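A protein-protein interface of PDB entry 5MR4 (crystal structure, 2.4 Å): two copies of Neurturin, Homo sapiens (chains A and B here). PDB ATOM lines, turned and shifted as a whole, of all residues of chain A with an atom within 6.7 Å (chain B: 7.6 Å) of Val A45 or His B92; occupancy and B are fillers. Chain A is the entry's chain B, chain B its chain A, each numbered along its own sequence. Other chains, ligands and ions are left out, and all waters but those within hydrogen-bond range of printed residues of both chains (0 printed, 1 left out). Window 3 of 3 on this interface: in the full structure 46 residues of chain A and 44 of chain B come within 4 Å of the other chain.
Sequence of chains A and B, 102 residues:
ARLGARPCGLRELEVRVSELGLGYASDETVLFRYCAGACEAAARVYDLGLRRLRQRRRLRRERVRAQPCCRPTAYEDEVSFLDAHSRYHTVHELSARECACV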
ATOM      1  N   ALA A  42       3.277 -14.975 -25.273  1.00  0.00           N
ATOM      2  CA  ALA A  42       4.209 -13.884 -25.480  1.00  0.00           C
ATOM      3  C   ALA A  42       4.078 -12.836 -24.369  1.00  0.00           C
ATOM      4  O   ALA A  42       2.977 -12.515 -23.923  1.00  0.00           O
ATOM      5  CB  ALA A  42       3.945 -13.214 -26.828  1.00  0.00           C
ATOM      6  N   ALA A  43       5.220 -12.301 -23.972  1.00  0.00           N
ATOM      7  CA  ALA A  43       5.303 -11.250 -22.998  1.00  0.00           C
ATOM      8  C   ALA A  43       4.529 -10.016 -23.451  1.00  0.00           C
ATOM      9  O   ALA A  43       4.627  -9.580 -24.611  1.00  0.00           O
ATOM     10  CB  ALA A  43       6.761 -10.886 -22.733  1.00  0.00           C
ATOM     11  N   ARG A  44       3.776  -9.465 -22.503  1.00  0.00           N
ATOM     12  CA  ARG A  44       3.037  -8.239 -22.688  1.00  0.00           C
ATOM     13  C   ARG A  44       3.979  -7.063 -22.703  1.00  0.00           C
ATOM     14  O   ARG A  44       5.017  -7.081 -22.003  1.00  0.00           O
ATOM     15  CB  ARG A  44       2.122  -8.034 -21.494  1.00  0.00           C
ATOM     16  CG  ARG A  44       0.948  -8.968 -21.406  1.00  0.00           C
ATOM     17  CD  ARG A  44       0.009  -8.510 -20.311  1.00  0.00           C
ATOM     18  NE  ARG A  44      -1.291  -9.101 -20.510  1.00  0.00           N
ATOM     19  CZ  ARG A  44      -2.263  -8.599 -21.258  1.00  0.00           C
ATOM     20  NH1 ARG A  44      -2.129  -7.426 -21.897  1.00  0.00           N
ATOM     21  NH2 ARG A  44      -3.396  -9.278 -21.343  1.00  0.00           N
ATOM     22  N   VAL A  45       3.583  -6.011 -23.423  1.00  0.00           N
ATOM     23  CA  VAL A  45       4.343  -4.767 -23.398  1.00  0.00           C
ATOM     24  C   VAL A  45       4.323  -4.171 -22.015  1.00  0.00           C
ATOM     25  O   VAL A  45       5.295  -3.594 -21.606  1.00  0.00           O
ATOM     26  CB  VAL A  45       3.883  -3.694 -24.420  1.00  0.00           C
ATOM     27  CG1 VAL A  45       4.269  -4.105 -25.817  1.00  0.00           C
ATOM     28  CG2 VAL A  45       2.410  -3.430 -24.338  1.00  0.00           C
ATOM     29  N   TYR A  46       3.199  -4.309 -21.316  1.00  0.00           N
ATOM     30  CA  TYR A  46       3.077  -3.905 -19.899  1.00  0.00           C
ATOM     31  C   TYR A  46       4.159  -4.526 -19.036  1.00  0.00           C
ATOM     32  O   TYR A  46       4.815  -3.835 -18.290  1.00  0.00           O
ATOM     33  CB  TYR A  46       1.698  -4.294 -19.352  1.00  0.00           C
ATOM     34  CG  TYR A  46       1.565  -4.208 -17.876  1.00  0.00           C
ATOM     35  CD1 TYR A  46       1.286  -3.022 -17.261  1.00  0.00           C
ATOM     36  CD2 TYR A  46       1.683  -5.345 -17.083  1.00  0.00           C
ATOM     37  CE1 TYR A  46       1.134  -2.940 -15.888  1.00  0.00           C
ATOM     38  CE2 TYR A  46       1.522  -5.282 -15.718  1.00  0.00           C
ATOM     39  CZ  TYR A  46       1.252  -4.071 -15.118  1.00  0.00           C
ATOM     40  OH  TYR A  46       1.109  -4.017 -13.750  1.00  0.00           O
ATOM     41  N   ASP A  47       4.347  -5.826 -19.157  1.00  0.00           N
ATOM     42  CA  ASP A  47       5.350  -6.519 -18.344  1.00  0.00           C
ATOM     43  C   ASP A  47       6.780  -6.159 -18.758  1.00  0.00           C
ATOM     44  O   ASP A  47       7.650  -6.000 -17.904  1.00  0.00           O
ATOM     45  CB  ASP A  47       5.127  -8.031 -18.378  1.00  0.00           C
ATOM     46  CG  ASP A  47       3.940  -8.465 -17.510  1.00  0.00           C
ATOM     47  OD1 ASP A  47       3.777  -7.877 -16.419  1.00  0.00           O
ATOM     48  OD2 ASP A  47       3.169  -9.383 -17.902  1.00  0.00           O
ATOM     49  N   LEU A  48       7.017  -6.001 -20.060  1.00  0.00           N
ATOM     50  CA  LEU A  48       8.346  -5.609 -20.548  1.00  0.00           C
ATOM     51  C   LEU A  48       8.701  -4.201 -20.047  1.00  0.00           C
ATOM     52  O   LEU A  48       9.812  -3.937 -19.566  1.00  0.00           O
ATOM     53  CB  LEU A  48       8.407  -5.694 -22.072  1.00  0.00           C
ATOM     54  CG  LEU A  48       8.985  -6.902 -22.791  1.00  0.00           C
ATOM     55  CD1 LEU A  48       9.320  -8.106 -21.940  1.00  0.00           C
ATOM     56  CD2 LEU A  48       8.113  -7.298 -23.959  1.00  0.00           C
ATOM     57  N   GLY A  49       7.727  -3.315 -20.110  1.00  0.00           N
ATOM     58  CA  GLY A  49       7.860  -1.971 -19.524  1.00  0.00           C
ATOM     59  C   GLY A  49       8.183  -1.994 -18.039  1.00  0.00           C
ATOM     60  O   GLY A  49       9.086  -1.315 -17.552  1.00  0.00           O
ATOM     61  N   LEU A  50       7.410  -2.782 -17.324  1.00  0.00           N
ATOM     62  CA  LEU A  50       7.503  -2.883 -15.888  1.00  0.00           C
ATOM     63  C   LEU A  50       8.853  -3.495 -15.475  1.00  0.00           C
ATOM     64  O   LEU A  50       9.483  -3.013 -14.561  1.00  0.00           O
ATOM     65  CB  LEU A  50       6.337  -3.719 -15.380  1.00  0.00           C
ATOM     66  CG  LEU A  50       5.873  -3.640 -13.945  1.00  0.00           C
ATOM     67  CD1 LEU A  50       5.454  -2.232 -13.595  1.00  0.00           C
ATOM     68  CD2 LEU A  50       4.697  -4.586 -13.785  1.00  0.00           C
ATOM     69  N   LEU B  20      11.420   2.997 -21.689  1.00  0.00           N
ATOM     70  CA  LEU B  20      10.738   1.720 -21.512  1.00  0.00           C
ATOM     71  C   LEU B  20      11.407   0.487 -22.114  1.00  0.00           C
ATOM     72  O   LEU B  20      11.018  -0.655 -21.810  1.00  0.00           O
ATOM     73  CB  LEU B  20       9.297   1.831 -22.031  1.00  0.00           C
ATOM     74  CG  LEU B  20       8.427   2.776 -21.205  1.00  0.00           C
ATOM     75  CD1 LEU B  20       7.096   3.030 -21.853  1.00  0.00           C
ATOM     76  CD2 LEU B  20       8.195   2.221 -19.827  1.00  0.00           C
ATOM     77  N   LEU B  22      11.264  -0.382 -25.273  1.00  0.00           N
ATOM     78  CA  LEU B  22      10.347  -0.936 -26.272  1.00  0.00           C
ATOM     79  C   LEU B  22      10.640  -0.501 -27.702  1.00  0.00           C
ATOM     80  O   LEU B  22       9.895  -0.869 -28.609  1.00  0.00           O
ATOM     81  CB  LEU B  22       8.888  -0.637 -25.895  1.00  0.00           C
ATOM     82  CG  LEU B  22       8.465  -1.229 -24.545  1.00  0.00           C
ATOM     83  CD1 LEU B  22       7.091  -0.707 -24.161  1.00  0.00           C
ATOM     84  CD2 LEU B  22       8.464  -2.747 -24.535  1.00  0.00           C
ATOM     85  N   TYR B  24      11.040   2.645 -28.925  1.00  0.00           N
ATOM     86  CA  TYR B  24      10.499   3.939 -29.307  1.00  0.00           C
ATOM     87  C   TYR B  24      11.449   5.071 -28.970  1.00  0.00           C
ATOM     88  O   TYR B  24      11.583   5.482 -27.817  1.00  0.00           O
ATOM     89  CB  TYR B  24       9.154   4.172 -28.607  1.00  0.00           C
ATOM     90  CG  TYR B  24       8.143   3.085 -28.884  1.00  0.00           C
ATOM     91  CD1 TYR B  24       7.659   2.883 -30.179  1.00  0.00           C
ATOM     92  CD2 TYR B  24       7.673   2.257 -27.858  1.00  0.00           C
ATOM     93  CE1 TYR B  24       6.744   1.876 -30.456  1.00  0.00           C
ATOM     94  CE2 TYR B  24       6.777   1.242 -28.126  1.00  0.00           C
ATOM     95  CZ  TYR B  24       6.302   1.070 -29.423  1.00  0.00           C
ATOM     96  OH  TYR B  24       5.394   0.086 -29.699  1.00  0.00           O
ATOM     97  N   PHE B  32       2.157   5.961 -17.101  1.00  0.00           N
ATOM     98  CA  PHE B  32       2.208   4.532 -16.950  1.00  0.00           C
ATOM     99  C   PHE B  32       1.525   4.102 -15.646  1.00  0.00           C
ATOM    100  O   PHE B  32       1.948   4.477 -14.561  1.00  0.00           O
ATOM    101  CB  PHE B  32       3.668   4.102 -16.952  1.00  0.00           C
ATOM    102  CG  PHE B  32       3.856   2.639 -16.908  1.00  0.00           C
ATOM    103  CD1 PHE B  32       3.588   1.864 -18.016  1.00  0.00           C
ATOM    104  CD2 PHE B  32       4.321   2.022 -15.744  1.00  0.00           C
ATOM    105  CE1 PHE B  32       3.771   0.483 -17.981  1.00  0.00           C
ATOM    106  CE2 PHE B  32       4.516   0.655 -15.705  1.00  0.00           C
ATOM    107  CZ  PHE B  32       4.225  -0.112 -16.819  1.00  0.00           C
ATOM    108  N   TYR B  75      -6.625  -3.586 -19.115  1.00  0.00           N
ATOM    109  CA  TYR B  75      -5.519  -2.795 -19.618  1.00  0.00           C
ATOM    110  C   TYR B  75      -6.053  -1.571 -20.363  1.00  0.00           C
ATOM    111  O   TYR B  75      -7.172  -1.576 -20.860  1.00  0.00           O
ATOM    112  CB  TYR B  75      -4.680  -3.677 -20.536  1.00  0.00           C
ATOM    113  CG  TYR B  75      -3.904  -4.750 -19.793  1.00  0.00           C
ATOM    114  CD1 TYR B  75      -2.627  -4.500 -19.302  1.00  0.00           C
ATOM    115  CD2 TYR B  75      -4.443  -6.011 -19.579  1.00  0.00           C
ATOM    116  CE1 TYR B  75      -1.934  -5.464 -18.587  1.00  0.00           C
ATOM    117  CE2 TYR B  75      -3.745  -6.995 -18.883  1.00  0.00           C
ATOM    118  CZ  TYR B  75      -2.491  -6.717 -18.389  1.00  0.00           C
ATOM    119  OH  TYR B  75      -1.796  -7.678 -17.691  1.00  0.00           O
ATOM    120  N   GLU B  76      -5.247  -0.516 -20.408  1.00  0.00           N
ATOM    121  CA  GLU B  76      -5.464   0.667 -21.262  1.00  0.00           C
ATOM    122  C   GLU B  76      -5.636   0.275 -22.726  1.00  0.00           C
ATOM    123  O   GLU B  76      -4.912  -0.574 -23.198  1.00  0.00           O
ATOM    124  CB  GLU B  76      -4.256   1.608 -21.105  1.00  0.00           C
ATOM    125  CG  GLU B  76      -4.119   2.721 -22.127  1.00  0.00           C
ATOM    126  CD  GLU B  76      -2.887   3.605 -21.870  1.00  0.00           C
ATOM    127  OE1 GLU B  76      -3.045   4.774 -21.467  1.00  0.00           O
ATOM    128  OE2 GLU B  76      -1.761   3.142 -22.057  1.00  0.00           O
ATOM    129  N   ASP B  77      -6.594   0.880 -23.430  1.00  0.00           N
ATOM    130  CA  ASP B  77      -6.851   0.597 -24.862  1.00  0.00           C
ATOM    131  C   ASP B  77      -5.658   0.943 -25.735  1.00  0.00           C
ATOM    132  O   ASP B  77      -5.142   0.096 -26.473  1.00  0.00           O
ATOM    133  CB  ASP B  77      -8.042   1.412 -25.401  1.00  0.00           C
ATOM    134  CG  ASP B  77      -9.390   0.870 -24.967  1.00  0.00           C
ATOM    135  OD1 ASP B  77      -9.500  -0.302 -24.499  1.00  0.00           O
ATOM    136  OD2 ASP B  77     -10.363   1.641 -25.108  1.00  0.00           O
ATOM    137  N   GLU B  78      -5.238   2.198 -25.649  1.00  0.00           N
ATOM    138  CA  GLU B  78      -4.157   2.699 -26.498  1.00  0.00           C
ATOM    139  C   GLU B  78      -3.595   4.029 -26.046  1.00  0.00           C
ATOM    140  O   GLU B  78      -4.292   4.840 -25.447  1.00  0.00           O
ATOM    141  CB  GLU B  78      -4.609   2.810 -27.968  1.00  0.00           C
ATOM    142  CG  GLU B  78      -5.922   3.548 -28.212  1.00  0.00           C
ATOM    143  CD  GLU B  78      -6.191   3.722 -29.712  1.00  0.00           C
ATOM    144  OE1 GLU B  78      -5.846   4.793 -30.264  1.00  0.00           O
ATOM    145  OE2 GLU B  78      -6.685   2.759 -30.358  1.00  0.00           O
ATOM    146  N   VAL B  79      -2.321   4.240 -26.348  1.00  0.00           N
ATOM    147  CA  VAL B  79      -1.673   5.535 -26.174  1.00  0.00           C
ATOM    148  C   VAL B  79      -0.791   5.772 -27.413  1.00  0.00           C
ATOM    149  O   VAL B  79      -0.255   4.838 -28.010  1.00  0.00           O
ATOM    150  CB  VAL B  79      -0.903   5.601 -24.833  1.00  0.00           C
ATOM    151  CG1 VAL B  79       0.268   4.635 -24.798  1.00  0.00           C
ATOM    152  CG2 VAL B  79      -0.413   7.012 -24.554  1.00  0.00           C
ATOM    153  N   SER B  80      -0.651   7.020 -27.809  1.00  0.00           N
ATOM    154  CA  SER B  80       0.122   7.349 -28.999  1.00  0.00           C
ATOM    155  C   SER B  80       1.122   8.457 -28.708  1.00  0.00           C
ATOM    156  O   SER B  80       0.987   9.216 -27.739  1.00  0.00           O
ATOM    157  CB  SER B  80      -0.798   7.780 -30.150  1.00  0.00           C
ATOM    158  OG  SER B  80      -1.610   6.718 -30.643  1.00  0.00           O
ATOM    159  N   THR B  90       1.310   4.049 -32.024  1.00  0.00           N
ATOM    160  CA  THR B  90       0.244   3.717 -31.096  1.00  0.00           C
ATOM    161  C   THR B  90       0.573   2.399 -30.404  1.00  0.00           C
ATOM    162  O   THR B  90       0.867   1.439 -31.084  1.00  0.00           O
ATOM    163  CB  THR B  90      -1.090   3.555 -31.796  1.00  0.00           C
ATOM    164  OG1 THR B  90      -1.375   4.748 -32.501  1.00  0.00           O
ATOM    165  CG2 THR B  90      -2.196   3.344 -30.762  1.00  0.00           C
ATOM    166  N   VAL B  91       0.522   2.378 -29.067  1.00  0.00           N
ATOM    167  CA  VAL B  91       0.782   1.171 -28.275  1.00  0.00           C
ATOM    168  C   VAL B  91      -0.492   0.766 -27.563  1.00  0.00           C
ATOM    169  O   VAL B  91      -1.145   1.577 -26.923  1.00  0.00           O
ATOM    170  CB  VAL B  91       1.913   1.374 -27.259  1.00  0.00           C
ATOM    171  CG1 VAL B  91       2.267   0.057 -26.584  1.00  0.00           C
ATOM    172  CG2 VAL B  91       3.152   1.864 -27.980  1.00  0.00           C
ATOM    173  N   HIS B  92      -0.829  -0.505 -27.687  1.00  0.00           N
ATOM    174  CA  HIS B  92      -2.015  -1.088 -27.058  1.00  0.00           C
ATOM    175  C   HIS B  92      -1.639  -1.790 -25.759  1.00  0.00           C
ATOM    176  O   HIS B  92      -0.607  -2.457 -25.686  1.00  0.00           O
ATOM    177  CB  HIS B  92      -2.707  -2.050 -28.026  1.00  0.00           C
ATOM    178  CG  HIS B  92      -3.088  -1.404 -29.316  1.00  0.00           C
ATOM    179  ND1 HIS B  92      -4.339  -0.865 -29.541  1.00  0.00           N
ATOM    180  CD2 HIS B  92      -2.363  -1.161 -30.437  1.00  0.00           C
ATOM    181  CE1 HIS B  92      -4.369  -0.327 -30.749  1.00  0.00           C
ATOM    182  NE2 HIS B  92      -3.186  -0.499 -31.314  1.00  0.00           N
ATOM    183  N   GLU B  93      -2.459  -1.578 -24.730  1.00  0.00           N
ATOM    184  CA  GLU B  93      -2.340  -2.300 -23.448  1.00  0.00           C
ATOM    185  C   GLU B  93      -0.994  -2.121 -22.778  1.00  0.00           C
ATOM    186  O   GLU B  93      -0.425  -3.069 -22.200  1.00  0.00           O
ATOM    187  CB  GLU B  93      -2.670  -3.787 -23.639  1.00  0.00           C
ATOM    188  CG  GLU B  93      -4.022  -4.011 -24.277  1.00  0.00           C
ATOM    189  CD  GLU B  93      -4.574  -5.410 -24.076  1.00  0.00           C
ATOM    190  OE1 GLU B  93      -3.841  -6.393 -24.244  1.00  0.00           O
ATOM    191  OE2 GLU B  93      -5.768  -5.528 -23.760  1.00  0.00           O
ATOM    192  N   LEU B  94      -0.469  -0.907 -22.853  1.00  0.00           N
ATOM    193  CA  LEU B  94       0.820  -0.600 -22.220  1.00  0.00           C
ATOM    194  C   LEU B  94       0.668  -0.481 -20.708  1.00  0.00           C
ATOM    195  O   LEU B  94       1.559  -0.901 -19.981  1.00  0.00           O
ATOM    196  CB  LEU B  94       1.427   0.667 -22.784  1.00  0.00           C
ATOM    197  CG  LEU B  94       2.732   1.158 -22.139  1.00  0.00           C
ATOM    198  CD1 LEU B  94       3.837   0.125 -22.230  1.00  0.00           C
ATOM    199  CD2 LEU B  94       3.174   2.463 -22.779  1.00  0.00           C
ATOM    200  N   SER B  95      -0.449   0.121 -20.274  1.00  0.00           N
ATOM    201  CA  SER B  95      -0.769   0.391 -18.861  1.00  0.00           C
ATOM    202  C   SER B  95      -1.903  -0.462 -18.357  1.00  0.00           C
ATOM    203  O   SER B  95      -2.765  -0.864 -19.135  1.00  0.00           O
ATOM    204  CB  SER B  95      -1.197   1.841 -18.657  1.00  0.00           C
ATOM    205  OG  SER B  95      -0.085   2.695 -18.491  1.00  0.00           O
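NE of Arg A44 is in hydrogen-bond range of OH of Tyr B75 (3.2 Å). The side-chain carboxylate of Glu B93 lies within salt-bridge range of the guanidinium group of Arg A44, at 3.1 Å.
N of Glu B93 lies within hydrogen-bond range of O of Glu B76 (3.1 Å). The backbone carbonyl oxygen (O) of Asp B77 is in hydrogen-bond range of a ring nitrogen (ND1) of His B92, at 3.3 Å.
Among the printed residues, merely in contact across the chains: Tyr A46 with Leu B94, Val A45 with His B92, Val A45 with Glu B93, Leu A50 with Phe B32, Tyr A46 with Glu B93, Tyr A46 with Tyr B75, Leu A48 with Leu B22 and Val A45 with Leu B94.
Of chain B, only His B92 (3.4 Å), Glu B93 (3.6 Å) and Leu B94 (3.9 Å) come within 4 Å of Val A45. His B92 touches just one residue of chain A: Val A45. Of the printed residues of chain B, Arg A44 touches Tyr B75 and Glu B93. Printed residues of chain A within 4 Å of Tyr B75: Arg A44 and Tyr A46. Gly A49 touches none of the printed residues of chain B. The nearest residue of chain B that does not touch Val A45 is Val B91 (4.2 Å). The nearest printed residue of chain A that does not touch Glu B93 is Asp A47 (6.3 Å).
Printed residues of chain B that touch a printed residue of chain A: Leu B22, Phe B32, Tyr B75, His B92, Glu B93 and Leu B94. Hydrophobic or aromatic side chains of chain B within 4 Å of the printed part of chain A: Leu B22, Phe B32 and Tyr B75. Printed residues of chain A that touch a printed residue of chain B: Arg A44, Val A45, Tyr A46, Leu A48 and Leu A50. Hydrophobic or aromatic side chains of chain A that line the printed part of chain B: Val A45, Tyr A46, Leu A48 and Leu A50. Among the printed residues, 10 pairs touch across the chains. Among the printed residues, Asp or Glu carboxylates within 4 Å of a Lys or Arg side-chain nitrogen of the other chain: Arg A44 with Glu B93.
No position is printed for both chains. Of the 10 pairs that touch across the chains among the printed residues, none has its exchanged pair printed and touching as well.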
